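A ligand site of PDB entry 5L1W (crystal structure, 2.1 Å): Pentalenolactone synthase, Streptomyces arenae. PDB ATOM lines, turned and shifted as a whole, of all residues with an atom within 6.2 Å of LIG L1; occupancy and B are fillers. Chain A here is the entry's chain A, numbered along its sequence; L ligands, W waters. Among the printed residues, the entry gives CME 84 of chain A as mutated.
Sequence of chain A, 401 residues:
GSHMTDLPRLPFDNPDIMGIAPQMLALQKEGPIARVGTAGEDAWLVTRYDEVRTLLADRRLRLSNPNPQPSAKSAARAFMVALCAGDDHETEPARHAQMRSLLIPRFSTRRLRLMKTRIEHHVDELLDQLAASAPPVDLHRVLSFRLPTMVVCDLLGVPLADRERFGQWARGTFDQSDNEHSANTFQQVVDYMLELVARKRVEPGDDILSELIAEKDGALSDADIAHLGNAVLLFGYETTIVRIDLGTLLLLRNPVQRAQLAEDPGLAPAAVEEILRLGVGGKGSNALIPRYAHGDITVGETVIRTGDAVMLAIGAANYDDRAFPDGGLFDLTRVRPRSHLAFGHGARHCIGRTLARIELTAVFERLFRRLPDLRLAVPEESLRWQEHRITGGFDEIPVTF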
ATOM      1  N   ARG A  77     -17.049 -28.875   9.352  1.00  0.00           N
ATOM      2  CA  ARG A  77     -15.860 -28.350  10.035  1.00  0.00           C
ATOM      3  C   ARG A  77     -14.789 -27.954   9.036  1.00  0.00           C
ATOM      4  O   ARG A  77     -14.053 -26.984   9.264  1.00  0.00           O
ATOM      5  CB  ARG A  77     -15.315 -29.371  11.023  1.00  0.00           C
ATOM      6  CG  ARG A  77     -16.016 -29.375  12.368  1.00  0.00           C
ATOM      7  CD  ARG A  77     -15.705 -28.109  13.170  1.00  0.00           C
ATOM      8  NE  ARG A  77     -16.404 -28.098  14.443  1.00  0.00           N
ATOM      9  CZ  ARG A  77     -16.380 -27.090  15.315  1.00  0.00           C
ATOM     10  NH1 ARG A  77     -15.683 -25.990  15.048  1.00  0.00           N
ATOM     11  NH2 ARG A  77     -17.042 -27.187  16.443  1.00  0.00           N
ATOM     12  N   MET A  80     -15.720 -24.568   7.682  1.00  0.00           N
ATOM     13  CA  MET A  80     -15.514 -23.532   8.683  1.00  0.00           C
ATOM     14  C   MET A  80     -14.038 -23.195   8.834  1.00  0.00           C
ATOM     15  O   MET A  80     -13.670 -22.021   8.937  1.00  0.00           O
ATOM     16  CB  MET A  80     -16.093 -23.979  10.023  1.00  0.00           C
ATOM     17  CG  MET A  80     -15.896 -22.953  11.128  1.00  0.00           C
ATOM     18  SD  MET A  80     -16.924 -23.315  12.545  1.00  0.00           S
ATOM     19  CE  MET A  80     -18.521 -22.761  11.945  1.00  0.00           C
ATOM     20  N   CME A  84     -11.846 -19.680   7.649  1.00  0.00           N
ATOM     21  CA  CME A  84     -11.052 -18.989   8.661  1.00  0.00           C
ATOM     22  CB  CME A  84     -11.285 -19.470  10.103  1.00  0.00           C
ATOM     23  SG  CME A  84     -12.810 -18.913  10.801  1.00  0.00           S
ATOM     24  SD  CME A  84     -12.554 -18.803  12.896  1.00  0.00           S
ATOM     25  CE  CME A  84     -13.239 -20.277  13.593  1.00  0.00           C
ATOM     26  CZ  CME A  84     -12.818 -21.553  12.895  1.00  0.00           C
ATOM     27  OH  CME A  84     -13.400 -22.640  13.609  1.00  0.00           O
ATOM     28  C   CME A  84      -9.558 -19.054   8.326  1.00  0.00           C
ATOM     29  O   CME A  84      -8.678 -18.746   9.133  1.00  0.00           O
ATOM     30  N   PHE A 174     -23.044 -25.789   8.008  1.00  0.00           N
ATOM     31  CA  PHE A 174     -22.449 -26.282   9.232  1.00  0.00           C
ATOM     32  C   PHE A 174     -23.221 -27.469   9.821  1.00  0.00           C
ATOM     33  O   PHE A 174     -23.138 -27.725  11.025  1.00  0.00           O
ATOM     34  CB  PHE A 174     -22.320 -25.139  10.233  1.00  0.00           C
ATOM     35  CG  PHE A 174     -21.501 -23.989   9.728  1.00  0.00           C
ATOM     36  CD1 PHE A 174     -20.378 -24.239   8.948  1.00  0.00           C
ATOM     37  CD2 PHE A 174     -21.840 -22.684   9.994  1.00  0.00           C
ATOM     38  CE1 PHE A 174     -19.609 -23.192   8.446  1.00  0.00           C
ATOM     39  CE2 PHE A 174     -21.082 -21.632   9.503  1.00  0.00           C
ATOM     40  CZ  PHE A 174     -19.963 -21.895   8.724  1.00  0.00           C
ATOM     41  N   LEU A 234     -21.741 -16.353   6.392  1.00  0.00           N
ATOM     42  CA  LEU A 234     -21.938 -17.565   7.175  1.00  0.00           C
ATOM     43  C   LEU A 234     -21.615 -17.379   8.655  1.00  0.00           C
ATOM     44  O   LEU A 234     -22.171 -18.113   9.483  1.00  0.00           O
ATOM     45  CB  LEU A 234     -21.096 -18.704   6.600  1.00  0.00           C
ATOM     46  CG  LEU A 234     -21.454 -19.157   5.177  1.00  0.00           C
ATOM     47  CD1 LEU A 234     -20.316 -19.930   4.505  1.00  0.00           C
ATOM     48  CD2 LEU A 234     -22.817 -19.891   5.153  1.00  0.00           C
ATOM     49  N   PHE A 235     -20.769 -16.416   9.017  1.00  0.00           N
ATOM     50  CA  PHE A 235     -20.546 -16.108  10.419  1.00  0.00           C
ATOM     51  C   PHE A 235     -21.359 -14.905  10.905  1.00  0.00           C
ATOM     52  O   PHE A 235     -21.437 -14.682  12.120  1.00  0.00           O
ATOM     53  CB  PHE A 235     -19.053 -15.825  10.691  1.00  0.00           C
ATOM     54  CG  PHE A 235     -18.113 -16.934  10.280  1.00  0.00           C
ATOM     55  CD1 PHE A 235     -18.531 -18.256  10.181  1.00  0.00           C
ATOM     56  CD2 PHE A 235     -16.782 -16.636  10.001  1.00  0.00           C
ATOM     57  CE1 PHE A 235     -17.653 -19.254   9.808  1.00  0.00           C
ATOM     58  CE2 PHE A 235     -15.891 -17.638   9.626  1.00  0.00           C
ATOM     59  CZ  PHE A 235     -16.326 -18.946   9.529  1.00  0.00           C
ATOM     60  N   THR A 239     -25.029 -16.947  14.574  1.00  0.00           N
ATOM     61  CA  THR A 239     -24.715 -16.942  16.002  1.00  0.00           C
ATOM     62  C   THR A 239     -25.429 -15.814  16.738  1.00  0.00           C
ATOM     63  O   THR A 239     -25.758 -15.961  17.920  1.00  0.00           O
ATOM     64  CB  THR A 239     -23.194 -16.843  16.225  1.00  0.00           C
ATOM     65  OG1 THR A 239     -22.674 -15.688  15.550  1.00  0.00           O
ATOM     66  CG2 THR A 239     -22.502 -18.093  15.702  1.00  0.00           C
ATOM     67  N   ARG A 243     -28.037 -15.895  19.991  1.00  0.00           N
ATOM     68  CA  ARG A 243     -27.902 -15.084  21.207  1.00  0.00           C
ATOM     69  C   ARG A 243     -29.165 -14.311  21.535  1.00  0.00           C
ATOM     70  O   ARG A 243     -29.456 -14.068  22.707  1.00  0.00           O
ATOM     71  CB  ARG A 243     -26.709 -14.127  21.121  1.00  0.00           C
ATOM     72  CG  ARG A 243     -25.380 -14.879  21.004  1.00  0.00           C
ATOM     73  CD  ARG A 243     -25.355 -16.185  21.862  1.00  0.00           C
ATOM     74  NE  ARG A 243     -24.107 -16.928  21.880  1.00  0.00           N
ATOM     75  CZ  ARG A 243     -23.757 -17.802  20.936  1.00  0.00           C
ATOM     76  NH1 ARG A 243     -24.484 -17.963  19.842  1.00  0.00           N
ATOM     77  NH2 ARG A 243     -22.640 -18.458  21.036  1.00  0.00           N
ATOM     78  N   SER A 285     -21.691 -27.665  22.648  1.00  0.00           N
ATOM     79  CA  SER A 285     -20.517 -28.001  21.841  1.00  0.00           C
ATOM     80  C   SER A 285     -19.985 -26.790  21.080  1.00  0.00           C
ATOM     81  O   SER A 285     -18.821 -26.793  20.680  1.00  0.00           O
ATOM     82  CB  SER A 285     -20.834 -29.126  20.853  1.00  0.00           C
ATOM     83  OG  SER A 285     -21.186 -30.321  21.530  1.00  0.00           O
ATOM     84  N   ASN A 286     -20.814 -25.761  20.864  1.00  0.00           N
ATOM     85  CA  ASN A 286     -20.381 -24.548  20.182  1.00  0.00           C
ATOM     86  C   ASN A 286     -19.665 -23.578  21.115  1.00  0.00           C
ATOM     87  O   ASN A 286     -19.011 -22.656  20.629  1.00  0.00           O
ATOM     88  CB  ASN A 286     -21.584 -23.850  19.527  1.00  0.00           C
ATOM     89  CG  ASN A 286     -22.588 -23.363  20.541  1.00  0.00           C
ATOM     90  OD1 ASN A 286     -23.075 -24.118  21.378  1.00  0.00           O
ATOM     91  ND2 ASN A 286     -22.913 -22.078  20.479  1.00  0.00           N
ATOM     92  N   ALA A 287     -19.784 -23.772  22.435  1.00  0.00           N
ATOM     93  CA  ALA A 287     -19.040 -22.993  23.421  1.00  0.00           C
ATOM     94  C   ALA A 287     -17.642 -23.561  23.671  1.00  0.00           C
ATOM     95  O   ALA A 287     -17.099 -23.436  24.779  1.00  0.00           O
ATOM     96  CB  ALA A 287     -19.823 -22.891  24.736  1.00  0.00           C
ATOM     97  N   LEU A 288     -17.053 -24.212  22.666  1.00  0.00           N
ATOM     98  CA  LEU A 288     -15.678 -24.680  22.712  1.00  0.00           C
ATOM     99  C   LEU A 288     -14.946 -24.129  21.494  1.00  0.00           C
ATOM    100  O   LEU A 288     -15.446 -24.232  20.367  1.00  0.00           O
ATOM    101  CB  LEU A 288     -15.597 -26.206  22.705  1.00  0.00           C
ATOM    102  CG  LEU A 288     -16.443 -27.035  23.670  1.00  0.00           C
ATOM    103  CD1 LEU A 288     -16.379 -28.504  23.267  1.00  0.00           C
ATOM    104  CD2 LEU A 288     -15.946 -26.859  25.079  1.00  0.00           C
ATOM    105  N   ILE A 289     -13.783 -23.527  21.721  1.00  0.00           N
ATOM    106  CA  ILE A 289     -12.923 -23.065  20.635  1.00  0.00           C
ATOM    107  C   ILE A 289     -11.851 -24.118  20.402  1.00  0.00           C
ATOM    108  O   ILE A 289     -11.065 -24.410  21.320  1.00  0.00           O
ATOM    109  CB  ILE A 289     -12.290 -21.702  20.948  1.00  0.00           C
ATOM    110  CG1 ILE A 289     -13.363 -20.616  20.967  1.00  0.00           C
ATOM    111  CG2 ILE A 289     -11.219 -21.384  19.922  1.00  0.00           C
ATOM    112  CD1 ILE A 289     -12.816 -19.231  21.305  1.00  0.00           C
ATOM    113  N   PRO A 290     -11.786 -24.729  19.214  1.00  0.00           N
ATOM    114  CA  PRO A 290     -10.801 -25.780  18.956  1.00  0.00           C
ATOM    115  C   PRO A 290      -9.462 -25.233  18.493  1.00  0.00           C
ATOM    116  O   PRO A 290      -9.376 -24.205  17.829  1.00  0.00           O
ATOM    117  CB  PRO A 290     -11.467 -26.603  17.846  1.00  0.00           C
ATOM    118  CG  PRO A 290     -12.233 -25.558  17.069  1.00  0.00           C
ATOM    119  CD  PRO A 290     -12.702 -24.535  18.079  1.00  0.00           C
ATOM    120  N   ILE A 314     -14.859 -21.896  26.354  1.00  0.00           N
ATOM    121  CA  ILE A 314     -15.206 -20.521  26.700  1.00  0.00           C
ATOM    122  C   ILE A 314     -16.512 -20.474  27.480  1.00  0.00           C
ATOM    123  O   ILE A 314     -16.694 -19.602  28.343  1.00  0.00           O
ATOM    124  CB  ILE A 314     -15.287 -19.646  25.431  1.00  0.00           C
ATOM    125  CG1 ILE A 314     -16.192 -20.290  24.387  1.00  0.00           C
ATOM    126  CG2 ILE A 314     -13.890 -19.379  24.887  1.00  0.00           C
ATOM    127  CD1 ILE A 314     -16.409 -19.428  23.143  1.00  0.00           C
ATOM    128  N   ALA A 342     -16.936 -14.985  25.407  1.00  0.00           N
ATOM    129  CA  ALA A 342     -17.885 -15.475  24.415  1.00  0.00           C
ATOM    130  C   ALA A 342     -17.540 -15.051  22.986  1.00  0.00           C
ATOM    131  O   ALA A 342     -18.023 -15.680  22.039  1.00  0.00           O
ATOM    132  CB  ALA A 342     -19.302 -14.992  24.772  1.00  0.00           C
ATOM    133  N   ILE A 390     -22.939 -26.968  13.919  1.00  0.00           N
ATOM    134  CA  ILE A 390     -21.803 -26.428  14.662  1.00  0.00           C
ATOM    135  C   ILE A 390     -22.256 -25.267  15.532  1.00  0.00           C
ATOM    136  O   ILE A 390     -21.784 -25.101  16.672  1.00  0.00           O
ATOM    137  CB  ILE A 390     -20.683 -26.000  13.704  1.00  0.00           C
ATOM    138  CG1 ILE A 390     -20.102 -27.205  12.965  1.00  0.00           C
ATOM    139  CG2 ILE A 390     -19.573 -25.271  14.454  1.00  0.00           C
ATOM    140  CD1 ILE A 390     -19.157 -26.832  11.847  1.00  0.00           C
ATOM    141  N   THR A 391     -23.197 -24.481  15.041  1.00  0.00           N
ATOM    142  CA  THR A 391     -23.697 -23.300  15.726  1.00  0.00           C
ATOM    143  C   THR A 391     -24.911 -23.593  16.614  1.00  0.00           C
ATOM    144  O   THR A 391     -25.482 -22.654  17.178  1.00  0.00           O
ATOM    145  CB  THR A 391     -24.031 -22.217  14.697  1.00  0.00           C
ATOM    146  OG1 THR A 391     -24.748 -22.798  13.607  1.00  0.00           O
ATOM    147  CG2 THR A 391     -22.757 -21.588  14.172  1.00  0.00           C
ATOM    148  N   GLY A 392     -25.310 -24.862  16.743  1.00  0.00           N
ATOM    149  CA  GLY A 392     -26.380 -25.229  17.649  1.00  0.00           C
ATOM    150  C   GLY A 392     -27.666 -24.479  17.342  1.00  0.00           C
ATOM    151  O   GLY A 392     -28.097 -24.390  16.196  1.00  0.00           O
HETATM  152  C1  LIG L   1     -17.634 -18.220  15.793  1.00  0.00           C
HETATM  153  C2  LIG L   1     -17.596 -19.041  14.506  1.00  0.00           C
HETATM  154  C3  LIG L   1     -16.637 -18.432  13.489  1.00  0.00           C
HETATM  155  C4  LIG L   1     -18.982 -19.105  13.841  1.00  0.00           C
HETATM  156  C5  LIG L   1     -18.901 -19.196  17.703  1.00  0.00           C
HETATM  157  C6  LIG L   1     -19.102 -22.514  16.960  1.00  0.00           C
HETATM  158  C7  LIG L   1     -16.477 -21.283  18.712  1.00  0.00           C
HETATM  159  C8  LIG L   1     -17.024 -20.392  15.014  1.00  0.00           C
HETATM  160  C9  LIG L   1     -20.914 -20.423  17.905  1.00  0.00           C
HETATM  161  C10 LIG L   1     -16.754 -22.820  16.755  1.00  0.00           C
HETATM  162  C11 LIG L   1     -19.684 -20.229  17.363  1.00  0.00           C
HETATM  163  C12 LIG L   1     -17.667 -19.205  17.006  1.00  0.00           C
HETATM  164  C13 LIG L   1     -19.059 -21.078  16.440  1.00  0.00           C
HETATM  165  C14 LIG L   1     -16.703 -21.521  17.246  1.00  0.00           C
HETATM  166  C15 LIG L   1     -17.607 -20.599  16.427  1.00  0.00           C
HETATM  167  O1  LIG L   1     -21.348 -19.621  18.756  1.00  0.00           O
HETATM  168  O2  LIG L   1     -15.722 -23.444  16.504  1.00  0.00           O
HETATM  169  O3  LIG L   1     -21.654 -21.367  17.555  1.00  0.00           O
HETATM  170  O4  LIG L   1     -17.997 -23.325  16.488  1.00  0.00           O
HETATM  171  O5  LIG L   1     -15.426 -21.053  17.702  1.00  0.00           O
HETATM  172  C1  LG2 L   2     -14.718 -15.194  15.281  1.00  0.00           C
HETATM  173  C2  LG2 L   2     -18.409 -15.564  18.423  1.00  0.00           C
HETATM  174  C3  LG2 L   2     -20.980 -12.467  15.695  1.00  0.00           C
HETATM  175  C4  LG2 L   2     -17.500 -12.460  12.340  1.00  0.00           C
HETATM  176  C5  LG2 L   2     -15.445 -15.525  16.399  1.00  0.00           C
HETATM  177  C6  LG2 L   2     -14.976 -16.267  17.553  1.00  0.00           C
HETATM  178  C7  LG2 L   2     -15.997 -16.363  18.420  1.00  0.00           C
HETATM  179  C8  LG2 L   2     -17.145 -15.675  17.846  1.00  0.00           C
HETATM  180  C9  LG2 L   2     -15.957 -17.073  19.791  1.00  0.00           C
HETATM  181  C10 LG2 L   2     -13.544 -16.840  17.786  1.00  0.00           C
HETATM  182  C11 LG2 L   2     -13.332 -18.163  17.067  1.00  0.00           C
HETATM  183  C12 LG2 L   2     -11.930 -18.686  17.334  1.00  0.00           C
HETATM  184  O1  LG2 L   2     -11.252 -18.173  18.282  1.00  0.00           O
HETATM  185  O2  LG2 L   2     -11.468 -19.627  16.617  1.00  0.00           O
HETATM  186  C13 LG2 L   2     -19.427 -14.750  17.964  1.00  0.00           C
HETATM  187  C14 LG2 L   2     -20.706 -14.516  18.611  1.00  0.00           C
HETATM  188  C15 LG2 L   2     -21.422 -13.671  17.853  1.00  0.00           C
HETATM  189  C16 LG2 L   2     -20.609 -13.318  16.708  1.00  0.00           C
HETATM  190  C17 LG2 L   2     -21.127 -15.186  19.941  1.00  0.00           C
HETATM  191  C18 LG2 L   2     -22.835 -13.090  18.083  1.00  0.00           C
HETATM  192  C19 LG2 L   2     -23.316 -12.811  19.307  1.00  0.00           C
HETATM  193  C20 LG2 L   2     -20.280 -12.182  14.553  1.00  0.00           C
HETATM  194  C21 LG2 L   2     -20.698 -11.307  13.487  1.00  0.00           C
HETATM  195  C22 LG2 L   2     -19.729 -11.290  12.551  1.00  0.00           C
HETATM  196  C23 LG2 L   2     -18.676 -12.175  13.006  1.00  0.00           C
HETATM  197  C24 LG2 L   2     -22.033 -10.531  13.513  1.00  0.00           C
HETATM  198  C25 LG2 L   2     -19.643 -10.529  11.196  1.00  0.00           C
HETATM  199  C26 LG2 L   2     -20.660  -9.844  10.640  1.00  0.00           C
HETATM  200  C27 LG2 L   2     -16.464 -13.233  12.824  1.00  0.00           C
HETATM  201  C28 LG2 L   2     -15.278 -13.610  12.088  1.00  0.00           C
HETATM  202  C29 LG2 L   2     -14.516 -14.368  12.896  1.00  0.00           C
HETATM  203  C30 LG2 L   2     -15.180 -14.495  14.168  1.00  0.00           C
HETATM  204  C31 LG2 L   2     -14.969 -13.214  10.636  1.00  0.00           C
HETATM  205  C32 LG2 L   2     -13.147 -14.986  12.522  1.00  0.00           C
HETATM  206  C33 LG2 L   2     -12.039 -14.235  13.262  1.00  0.00           C
HETATM  207  C34 LG2 L   2     -10.682 -14.841  12.972  1.00  0.00           C
HETATM  208  O3  LG2 L   2      -9.689 -14.078  12.989  1.00  0.00           O
HETATM  209  O4  LG2 L   2     -10.610 -16.077  12.690  1.00  0.00           O
HETATM  210  N1  LG2 L   2     -16.761 -15.186  16.611  1.00  0.00           N
HETATM  211  N2  LG2 L   2     -19.412 -14.001  16.795  1.00  0.00           N
HETATM  212  N3  LG2 L   2     -19.041 -12.710  14.220  1.00  0.00           N
HETATM  213  N4  LG2 L   2     -16.361 -13.794  14.088  1.00  0.00           N
HETATM  214 FE1  LG2 L   2     -17.784 -13.718  15.559  1.00  0.00          FE
HETATM  215  O   HOH W   1     -13.051 -22.085  15.996  1.00  0.00           O
HETATM  216  O   HOH W   2     -16.877 -25.791  18.740  1.00  0.00           O
HETATM  217  O   HOH W   3     -24.327 -20.161  17.976  1.00  0.00           O
HETATM  218  O   HOH W   4     -19.256 -19.758  20.858  1.00  0.00           O
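SD of Met 80 touches C8 of LIG L1 (3.8 Å).
CME 84 touches LIG L1 (OH to O2, 3.8 Å).
CD1 of Phe 235 touches C4 of LIG L1, at 3.8 Å.
Thr 239 touches LIG L1 (CG2 to C9, 3.6 Å).
Leu 288 touches LIG L1.
Ile 289 touches LIG L1 (CG1 to O5, 3.9 Å).
CD of Pro 290 touches O2 of LIG L1, 3.6 Å away.
Ile 390 touches LIG L1.
CA of Thr 391 touches O3 of LIG L1, 3.4 Å away.
Hydrophobic or aromatic side chains within 4 Å of LIG L1: Met 80, Phe 235, Ile 289, Pro 290 and Ile 390.
Along chain A the residues within 4 Å of LIG L1 span positions 77 to 391.
The nearest printed residue that does not touch LIG L1 is Ile 314 (4.8 Å).
The backbone NH (N) of Ile 390 sits at hydrogen-bond distance from the backbone carbonyl oxygen (O) of Phe 174, 3.0 Å away.
The side-chain sulfur of Met 80 lies close to OH of CME 84.
The guanidinium group (NH1) of Arg 243 is in hydrogen-bond range of the backbone carbonyl oxygen (O) of Thr 239, at 3.1 Å.
Water W3 lies within hydrogen-bond range of O of Thr 391 (2.9 Å), NH1 of Arg 243 (2.9 Å), O3 of LIG L1 (3.0 Å) and ND2 of Asn 286 (3.5 Å).
Water W4 bridges O of Asn 286 (2.9 Å) and O1 of LIG L1 (3.0 Å).
Water W1 lies within hydrogen-bond range of OH of CME 84, an oxygen (O2) of LG2 L2 and an oxygen (O2) of LIG L1.
ND2 of Asn 286 lies close to O3 of LIG L1 (3.3 Å).
O2 of LIG L1 sits at hydrogen-bond distance from NH1 of Arg 77, 2.9 Å away.
O1 of LIG L1 lies within salt-bridge range of NH2 of Arg 243 (2.9 Å).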
